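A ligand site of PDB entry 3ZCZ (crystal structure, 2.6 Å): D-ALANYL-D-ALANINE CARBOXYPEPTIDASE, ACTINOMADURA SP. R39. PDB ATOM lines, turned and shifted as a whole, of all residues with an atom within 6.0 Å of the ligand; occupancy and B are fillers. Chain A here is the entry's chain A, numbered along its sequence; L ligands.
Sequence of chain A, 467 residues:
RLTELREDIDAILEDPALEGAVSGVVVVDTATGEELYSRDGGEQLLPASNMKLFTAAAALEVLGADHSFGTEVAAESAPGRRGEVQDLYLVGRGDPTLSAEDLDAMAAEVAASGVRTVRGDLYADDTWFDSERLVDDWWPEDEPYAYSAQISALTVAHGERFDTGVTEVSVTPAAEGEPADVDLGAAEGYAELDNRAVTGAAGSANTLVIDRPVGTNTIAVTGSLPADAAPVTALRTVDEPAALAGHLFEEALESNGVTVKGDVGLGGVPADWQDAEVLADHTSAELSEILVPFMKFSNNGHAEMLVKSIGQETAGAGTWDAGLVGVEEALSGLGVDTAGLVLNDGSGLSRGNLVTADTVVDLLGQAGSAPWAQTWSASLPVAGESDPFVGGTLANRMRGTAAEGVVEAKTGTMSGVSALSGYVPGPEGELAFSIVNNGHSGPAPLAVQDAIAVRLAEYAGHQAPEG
OG of Ser 415 sits at hydrogen-bond distance from O4 of the ligand (3.1 Å).
O3 of the ligand sits at hydrogen-bond distance from N of Thr 413, 2.6 Å away.
The backbone NH (N) of Ser 415 is in hydrogen-bond range of an oxygen (O4) of the ligand, at 3.2 Å.
The backbone carbonyl oxygen of Thr 413 is in hydrogen-bond range of a nitrogen (N1) of the ligand (3.1 Å).
N of Ser 49 sits at hydrogen-bond distance from O3 of the ligand, 2.9 Å away.
The guanidinium group (NH1) of Arg 351 is in salt-bridge range of an oxygen (O1) of the ligand, 2.9 Å away.
The side-chain carboxylate (OD2) of Asp 142 is in salt-bridge range of a nitrogen (N2) of the ligand, at 2.9 Å.
The side-chain hydroxyl (OG) of Ser 49 is bonded to a carbon (C4) of the ligand (1.3 Å).
ND2 of Asn 300 sits at hydrogen-bond distance from O2 of the ligand (3.3 Å).
OG of Ser 298 sits at hydrogen-bond distance from NZ of Lys 52 (2.8 Å).
OG of Ser 298 sits close to OG of Ser 49 (3.2 Å).
OD1 of Asn 300 lies within hydrogen-bond range of NZ of Lys 52.
NZ of Lys 410 lies within hydrogen-bond range of OG of Ser 298.
The backbone NH of Leu 349 is in hydrogen-bond range of the side-chain hydroxyl of Ser 347.
The backbone carbonyl oxygen (O) of Ser 415 is in hydrogen-bond range of the guanidinium group (NH2) of Arg 351.
O of Tyr 147 lies within hydrogen-bond range of ND2 of Asn 300 (2.7 Å).
The backbone carbonyl oxygen of Ser 347 is in hydrogen-bond range of the side-chain amino group of Lys 52, at 3.1 Å.
F2 of the ligand lies close to OG of Ser 298 (2.9 Å).
Merely in contact with the ligand: Trp 139, Ala 48, Gly 412, Tyr 147, Leu 349, Met 414, Gly 348, Ser 347 and Lys 52.
Hydrophobic or aromatic side chains that line the ligand: Ala 48, Trp 139, Tyr 147, Leu 349 and Met 414.
16 residues have an atom within 4 Å of the ligand: Ala 48, Ser 49, Lys 52, Trp 139, Asp 142, Tyr 147, Ser 298, Asn 300, Ser 347, Gly 348, Leu 349, Arg 351, Gly 412, Thr 413, Met 414 and Ser 415.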
ATOM      1  N   PRO A  47     -18.479  21.949  19.242  1.00  0.00           N
ATOM      2  CA  PRO A  47     -19.602  21.067  19.557  1.00  0.00           C
ATOM      3  C   PRO A  47     -19.789  19.858  18.645  1.00  0.00           C
ATOM      4  O   PRO A  47     -20.571  18.965  18.971  1.00  0.00           O
ATOM      5  CB  PRO A  47     -20.802  22.002  19.393  1.00  0.00           C
ATOM      6  CG  PRO A  47     -20.376  22.957  18.338  1.00  0.00           C
ATOM      7  CD  PRO A  47     -18.897  23.118  18.451  1.00  0.00           C
ATOM      8  N   ALA A  48     -19.082  19.837  17.517  1.00  0.00           N
ATOM      9  CA  ALA A  48     -19.419  18.952  16.389  1.00  0.00           C
ATOM     10  C   ALA A  48     -20.912  19.102  16.055  1.00  0.00           C
ATOM     11  O   ALA A  48     -21.425  20.218  16.021  1.00  0.00           O
ATOM     12  CB  ALA A  48     -19.030  17.508  16.677  1.00  0.00           C
ATOM     13  N   SER A  49     -21.609  17.990  15.870  1.00  0.00           N
ATOM     14  CA  SER A  49     -23.045  18.023  15.522  1.00  0.00           C
ATOM     15  C   SER A  49     -24.020  18.445  16.645  1.00  0.00           C
ATOM     16  O   SER A  49     -25.229  18.461  16.423  1.00  0.00           O
ATOM     17  CB  SER A  49     -23.477  16.681  14.912  1.00  0.00           C
ATOM     18  OG  SER A  49     -22.649  16.339  13.826  1.00  0.00           O
ATOM     19  N   ASN A  50     -23.496  18.792  17.821  1.00  0.00           N
ATOM     20  CA  ASN A  50     -24.347  19.414  18.844  1.00  0.00           C
ATOM     21  C   ASN A  50     -24.799  20.831  18.455  1.00  0.00           C
ATOM     22  O   ASN A  50     -25.719  21.388  19.046  1.00  0.00           O
ATOM     23  CB  ASN A  50     -23.675  19.411  20.222  1.00  0.00           C
ATOM     24  CG  ASN A  50     -23.886  18.109  20.975  1.00  0.00           C
ATOM     25  OD1 ASN A  50     -24.035  17.035  20.389  1.00  0.00           O
ATOM     26  ND2 ASN A  50     -23.888  18.199  22.293  1.00  0.00           N
ATOM     27  N   LYS A  52     -26.379  21.436  15.837  1.00  0.00           N
ATOM     28  CA  LYS A  52     -27.701  21.222  15.269  1.00  0.00           C
ATOM     29  C   LYS A  52     -28.834  21.473  16.264  1.00  0.00           C
ATOM     30  O   LYS A  52     -29.949  21.827  15.873  1.00  0.00           O
ATOM     31  CB  LYS A  52     -27.818  19.807  14.699  1.00  0.00           C
ATOM     32  CG  LYS A  52     -27.028  19.610  13.418  1.00  0.00           C
ATOM     33  CD  LYS A  52     -27.331  18.263  12.799  1.00  0.00           C
ATOM     34  CE  LYS A  52     -26.462  18.007  11.572  1.00  0.00           C
ATOM     35  NZ  LYS A  52     -25.087  17.610  11.966  1.00  0.00           N
ATOM     36  N   TRP A 139     -13.032  21.491   5.258  1.00  0.00           N
ATOM     37  CA  TRP A 139     -11.847  20.890   4.637  1.00  0.00           C
ATOM     38  C   TRP A 139     -12.126  20.316   3.247  1.00  0.00           C
ATOM     39  O   TRP A 139     -13.043  19.505   3.090  1.00  0.00           O
ATOM     40  CB  TRP A 139     -11.254  19.816   5.550  1.00  0.00           C
ATOM     41  CG  TRP A 139     -10.687  20.356   6.840  1.00  0.00           C
ATOM     42  CD1 TRP A 139     -10.502  21.663   7.168  1.00  0.00           C
ATOM     43  CD2 TRP A 139     -10.181  19.592   7.943  1.00  0.00           C
ATOM     44  NE1 TRP A 139      -9.937  21.772   8.424  1.00  0.00           N
ATOM     45  CE2 TRP A 139      -9.724  20.510   8.919  1.00  0.00           C
ATOM     46  CE3 TRP A 139     -10.074  18.216   8.204  1.00  0.00           C
ATOM     47  CZ2 TRP A 139      -9.168  20.106  10.137  1.00  0.00           C
ATOM     48  CZ3 TRP A 139      -9.525  17.805   9.422  1.00  0.00           C
ATOM     49  CH2 TRP A 139      -9.082  18.754  10.373  1.00  0.00           C
ATOM     50  N   ASP A 142     -12.660  16.569   2.682  1.00  0.00           N
ATOM     51  CA  ASP A 142     -13.989  16.061   3.054  1.00  0.00           C
ATOM     52  C   ASP A 142     -15.025  16.077   1.909  1.00  0.00           C
ATOM     53  O   ASP A 142     -15.970  15.284   1.901  1.00  0.00           O
ATOM     54  CB  ASP A 142     -14.550  16.840   4.254  1.00  0.00           C
ATOM     55  CG  ASP A 142     -13.751  16.626   5.525  1.00  0.00           C
ATOM     56  OD1 ASP A 142     -12.853  15.761   5.545  1.00  0.00           O
ATOM     57  OD2 ASP A 142     -14.023  17.338   6.514  1.00  0.00           O
ATOM     58  N   TYR A 147     -21.726  14.027   4.009  1.00  0.00           N
ATOM     59  CA  TYR A 147     -21.865  15.014   5.067  1.00  0.00           C
ATOM     60  C   TYR A 147     -21.242  16.358   4.683  1.00  0.00           C
ATOM     61  O   TYR A 147     -21.407  17.361   5.378  1.00  0.00           O
ATOM     62  CB  TYR A 147     -21.234  14.508   6.371  1.00  0.00           C
ATOM     63  CG  TYR A 147     -19.724  14.360   6.306  1.00  0.00           C
ATOM     64  CD1 TYR A 147     -18.897  15.475   6.394  1.00  0.00           C
ATOM     65  CD2 TYR A 147     -19.139  13.110   6.172  1.00  0.00           C
ATOM     66  CE1 TYR A 147     -17.529  15.346   6.329  1.00  0.00           C
ATOM     67  CE2 TYR A 147     -17.776  12.970   6.120  1.00  0.00           C
ATOM     68  CZ  TYR A 147     -16.973  14.099   6.195  1.00  0.00           C
ATOM     69  OH  TYR A 147     -15.609  13.972   6.140  1.00  0.00           O
ATOM     70  N   PHE A 297     -30.286  11.191  12.338  1.00  0.00           N
ATOM     71  CA  PHE A 297     -29.060  10.772  11.638  1.00  0.00           C
ATOM     72  C   PHE A 297     -28.038  11.892  11.485  1.00  0.00           C
ATOM     73  O   PHE A 297     -26.958  11.687  10.928  1.00  0.00           O
ATOM     74  CB  PHE A 297     -29.402  10.160  10.280  1.00  0.00           C
ATOM     75  CG  PHE A 297     -30.444   9.084  10.338  1.00  0.00           C
ATOM     76  CD1 PHE A 297     -30.188   7.880  10.996  1.00  0.00           C
ATOM     77  CD2 PHE A 297     -31.696   9.278   9.758  1.00  0.00           C
ATOM     78  CE1 PHE A 297     -31.157   6.887  11.056  1.00  0.00           C
ATOM     79  CE2 PHE A 297     -32.657   8.292   9.820  1.00  0.00           C
ATOM     80  CZ  PHE A 297     -32.394   7.095  10.478  1.00  0.00           C
ATOM     81  N   SER A 298     -28.394  13.086  11.975  1.00  0.00           N
ATOM     82  CA  SER A 298     -27.496  14.235  11.989  1.00  0.00           C
ATOM     83  C   SER A 298     -27.097  14.654  10.559  1.00  0.00           C
ATOM     84  O   SER A 298     -25.937  14.568  10.182  1.00  0.00           O
ATOM     85  CB  SER A 298     -26.259  13.943  12.853  1.00  0.00           C
ATOM     86  OG  SER A 298     -25.551  15.139  13.139  1.00  0.00           O
ATOM     87  N   ASN A 299     -28.083  15.110   9.791  1.00  0.00           N
ATOM     88  CA  ASN A 299     -27.878  15.455   8.380  1.00  0.00           C
ATOM     89  C   ASN A 299     -27.310  16.864   8.243  1.00  0.00           C
ATOM     90  O   ASN A 299     -27.988  17.844   8.583  1.00  0.00           O
ATOM     91  CB  ASN A 299     -29.208  15.311   7.615  1.00  0.00           C
ATOM     92  CG  ASN A 299     -29.041  15.354   6.121  1.00  0.00           C
ATOM     93  OD1 ASN A 299     -28.389  16.244   5.565  1.00  0.00           O
ATOM     94  ND2 ASN A 299     -29.656  14.388   5.432  1.00  0.00           N
ATOM     95  N   ASN A 300     -26.071  16.966   7.766  1.00  0.00           N
ATOM     96  CA  ASN A 300     -25.379  18.256   7.660  1.00  0.00           C
ATOM     97  C   ASN A 300     -26.073  19.210   6.670  1.00  0.00           C
ATOM     98  O   ASN A 300     -26.380  20.351   7.017  1.00  0.00           O
ATOM     99  CB  ASN A 300     -23.899  18.081   7.265  1.00  0.00           C
ATOM    100  CG  ASN A 300     -23.028  17.526   8.392  1.00  0.00           C
ATOM    101  OD1 ASN A 300     -23.425  17.450   9.554  1.00  0.00           O
ATOM    102  ND2 ASN A 300     -21.816  17.135   8.040  1.00  0.00           N
ATOM    103  N   SER A 347     -24.555  23.004  10.911  1.00  0.00           N
ATOM    104  CA  SER A 347     -24.393  21.566  11.055  1.00  0.00           C
ATOM    105  C   SER A 347     -23.415  21.207  12.154  1.00  0.00           C
ATOM    106  O   SER A 347     -23.513  20.137  12.730  1.00  0.00           O
ATOM    107  CB  SER A 347     -23.950  20.936   9.741  1.00  0.00           C
ATOM    108  OG  SER A 347     -22.643  21.336   9.369  1.00  0.00           O
ATOM    109  N   GLY A 348     -22.480  22.118  12.432  1.00  0.00           N
ATOM    110  CA  GLY A 348     -21.418  21.857  13.391  1.00  0.00           C
ATOM    111  C   GLY A 348     -20.177  21.288  12.738  1.00  0.00           C
ATOM    112  O   GLY A 348     -19.180  21.005  13.408  1.00  0.00           O
ATOM    113  N   LEU A 349     -20.232  21.113  11.413  1.00  0.00           N
ATOM    114  CA  LEU A 349     -19.076  20.656  10.656  1.00  0.00           C
ATOM    115  C   LEU A 349     -17.901  21.636  10.757  1.00  0.00           C
ATOM    116  O   LEU A 349     -16.746  21.214  10.766  1.00  0.00           O
ATOM    117  CB  LEU A 349     -19.440  20.384   9.187  1.00  0.00           C
ATOM    118  CG  LEU A 349     -18.319  19.908   8.249  1.00  0.00           C
ATOM    119  CD1 LEU A 349     -17.638  18.632   8.755  1.00  0.00           C
ATOM    120  CD2 LEU A 349     -18.828  19.711   6.829  1.00  0.00           C
ATOM    121  N   ARG A 351     -15.070  23.839  12.171  1.00  0.00           N
ATOM    122  CA  ARG A 351     -14.198  23.907  13.336  1.00  0.00           C
ATOM    123  C   ARG A 351     -14.072  25.349  13.836  1.00  0.00           C
ATOM    124  O   ARG A 351     -13.326  25.628  14.779  1.00  0.00           O
ATOM    125  CB  ARG A 351     -12.823  23.266  13.032  1.00  0.00           C
ATOM    126  CG  ARG A 351     -12.959  21.820  12.541  1.00  0.00           C
ATOM    127  CD  ARG A 351     -11.651  21.054  12.478  1.00  0.00           C
ATOM    128  NE  ARG A 351     -11.307  20.473  13.770  1.00  0.00           N
ATOM    129  CZ  ARG A 351     -11.410  19.184  14.076  1.00  0.00           C
ATOM    130  NH1 ARG A 351     -11.826  18.286  13.197  1.00  0.00           N
ATOM    131  NH2 ARG A 351     -11.067  18.800  15.304  1.00  0.00           N
ATOM    132  N   THR A 393     -28.411   7.957  15.743  1.00  0.00           N
ATOM    133  CA  THR A 393     -26.980   7.791  15.994  1.00  0.00           C
ATOM    134  C   THR A 393     -26.720   7.091  17.334  1.00  0.00           C
ATOM    135  O   THR A 393     -25.601   6.670  17.603  1.00  0.00           O
ATOM    136  CB  THR A 393     -26.243   9.143  15.975  1.00  0.00           C
ATOM    137  OG1 THR A 393     -26.823  10.020  16.944  1.00  0.00           O
ATOM    138  CG2 THR A 393     -26.318   9.782  14.595  1.00  0.00           C
ATOM    139  N   LYS A 410     -28.582  14.254  21.636  1.00  0.00           N
ATOM    140  CA  LYS A 410     -27.914  14.492  20.358  1.00  0.00           C
ATOM    141  C   LYS A 410     -26.430  14.196  20.456  1.00  0.00           C
ATOM    142  O   LYS A 410     -25.762  14.585  21.430  1.00  0.00           O
ATOM    143  CB  LYS A 410     -28.148  15.947  19.901  1.00  0.00           C
ATOM    144  CG  LYS A 410     -27.582  16.288  18.506  1.00  0.00           C
ATOM    145  CD  LYS A 410     -28.370  15.617  17.382  1.00  0.00           C
ATOM    146  CE  LYS A 410     -27.716  15.848  16.014  1.00  0.00           C
ATOM    147  NZ  LYS A 410     -26.430  15.100  15.840  1.00  0.00           N
ATOM    148  N   THR A 411     -25.902  13.508  19.438  1.00  0.00           N
ATOM    149  CA  THR A 411     -24.489  13.157  19.374  1.00  0.00           C
ATOM    150  C   THR A 411     -23.713  14.174  18.542  1.00  0.00           C
ATOM    151  O   THR A 411     -24.303  15.017  17.880  1.00  0.00           O
ATOM    152  CB  THR A 411     -24.278  11.745  18.784  1.00  0.00           C
ATOM    153  OG1 THR A 411     -24.785  11.685  17.448  1.00  0.00           O
ATOM    154  CG2 THR A 411     -24.963  10.703  19.633  1.00  0.00           C
ATOM    155  N   GLY A 412     -22.382  14.087  18.606  1.00  0.00           N
ATOM    156  CA  GLY A 412     -21.516  14.946  17.816  1.00  0.00           C
ATOM    157  C   GLY A 412     -20.115  14.371  17.787  1.00  0.00           C
ATOM    158  O   GLY A 412     -19.516  14.169  18.833  1.00  0.00           O
ATOM    159  N   THR A 413     -19.602  14.108  16.593  1.00  0.00           N
ATOM    160  CA  THR A 413     -18.312  13.442  16.453  1.00  0.00           C
ATOM    161  C   THR A 413     -17.513  13.886  15.229  1.00  0.00           C
ATOM    162  O   THR A 413     -18.009  13.839  14.100  1.00  0.00           O
ATOM    163  CB  THR A 413     -18.493  11.898  16.442  1.00  0.00           C
ATOM    164  OG1 THR A 413     -19.214  11.505  17.635  1.00  0.00           O
ATOM    165  CG2 THR A 413     -17.151  11.180  16.411  1.00  0.00           C
ATOM    166  N   MET A 414     -16.277  14.320  15.479  1.00  0.00           N
ATOM    167  CA  MET A 414     -15.245  14.544  14.449  1.00  0.00           C
ATOM    168  C   MET A 414     -13.918  14.093  15.049  1.00  0.00           C
ATOM    169  O   MET A 414     -13.901  13.554  16.163  1.00  0.00           O
ATOM    170  CB  MET A 414     -15.132  16.030  14.114  1.00  0.00           C
ATOM    171  CG  MET A 414     -16.263  16.598  13.309  1.00  0.00           C
ATOM    172  SD  MET A 414     -15.956  18.336  12.906  1.00  0.00           S
ATOM    173  CE  MET A 414     -15.845  19.066  14.545  1.00  0.00           C
ATOM    174  N   SER A 415     -12.811  14.326  14.349  1.00  0.00           N
ATOM    175  CA  SER A 415     -11.472  14.142  14.912  1.00  0.00           C
ATOM    176  C   SER A 415     -11.283  15.046  16.127  1.00  0.00           C
ATOM    177  O   SER A 415     -11.460  16.263  16.027  1.00  0.00           O
ATOM    178  CB  SER A 415     -10.389  14.458  13.886  1.00  0.00           C
ATOM    179  OG  SER A 415     -10.268  13.421  12.945  1.00  0.00           O
HETATM  180  N1  LIG L   1     -19.720  15.483  12.038  1.00  0.00           N
HETATM  181  O1  LIG L   1     -12.435  16.015  11.536  1.00  0.00           O
HETATM  182  C1  LIG L   1     -19.503  14.921  10.836  1.00  0.00           C
HETATM  183  O2  LIG L   1     -20.338  14.937   9.934  1.00  0.00           O
HETATM  184  C2  LIG L   1     -20.877  16.099  12.314  1.00  0.00           C
HETATM  185  C3  LIG L   1     -20.601  17.574  12.463  1.00  0.00           C
HETATM  186  C4  LIG L   1     -21.611  15.544  13.525  1.00  0.00           C
HETATM  187  C5  LIG L   1     -22.179  14.143  13.223  1.00  0.00           C
HETATM  188  F1  LIG L   1     -22.886  13.635  14.245  1.00  0.00           F
HETATM  189  F2  LIG L   1     -22.961  14.277  12.166  1.00  0.00           F
HETATM  190  F3  LIG L   1     -21.202  13.294  12.949  1.00  0.00           F
HETATM  191  C6  LIG L   1     -18.163  14.254  10.593  1.00  0.00           C
HETATM  192  C7  LIG L   1     -17.258  15.295   9.930  1.00  0.00           C
HETATM  193  O3  LIG L   1     -20.692  15.493  14.640  1.00  0.00           O
HETATM  194  C8  LIG L   1     -14.840  15.908   9.520  1.00  0.00           C
HETATM  195  C9  LIG L   1     -13.404  15.386   9.455  1.00  0.00           C
HETATM  196  C10 LIG L   1     -15.868  14.789   9.583  1.00  0.00           C
HETATM  197  O4  LIG L   1     -12.852  13.888  11.212  1.00  0.00           O
HETATM  198  C11 LIG L   1     -12.865  15.073  10.828  1.00  0.00           C
HETATM  199  N2  LIG L   1     -12.551  16.404   8.857  1.00  0.00           N
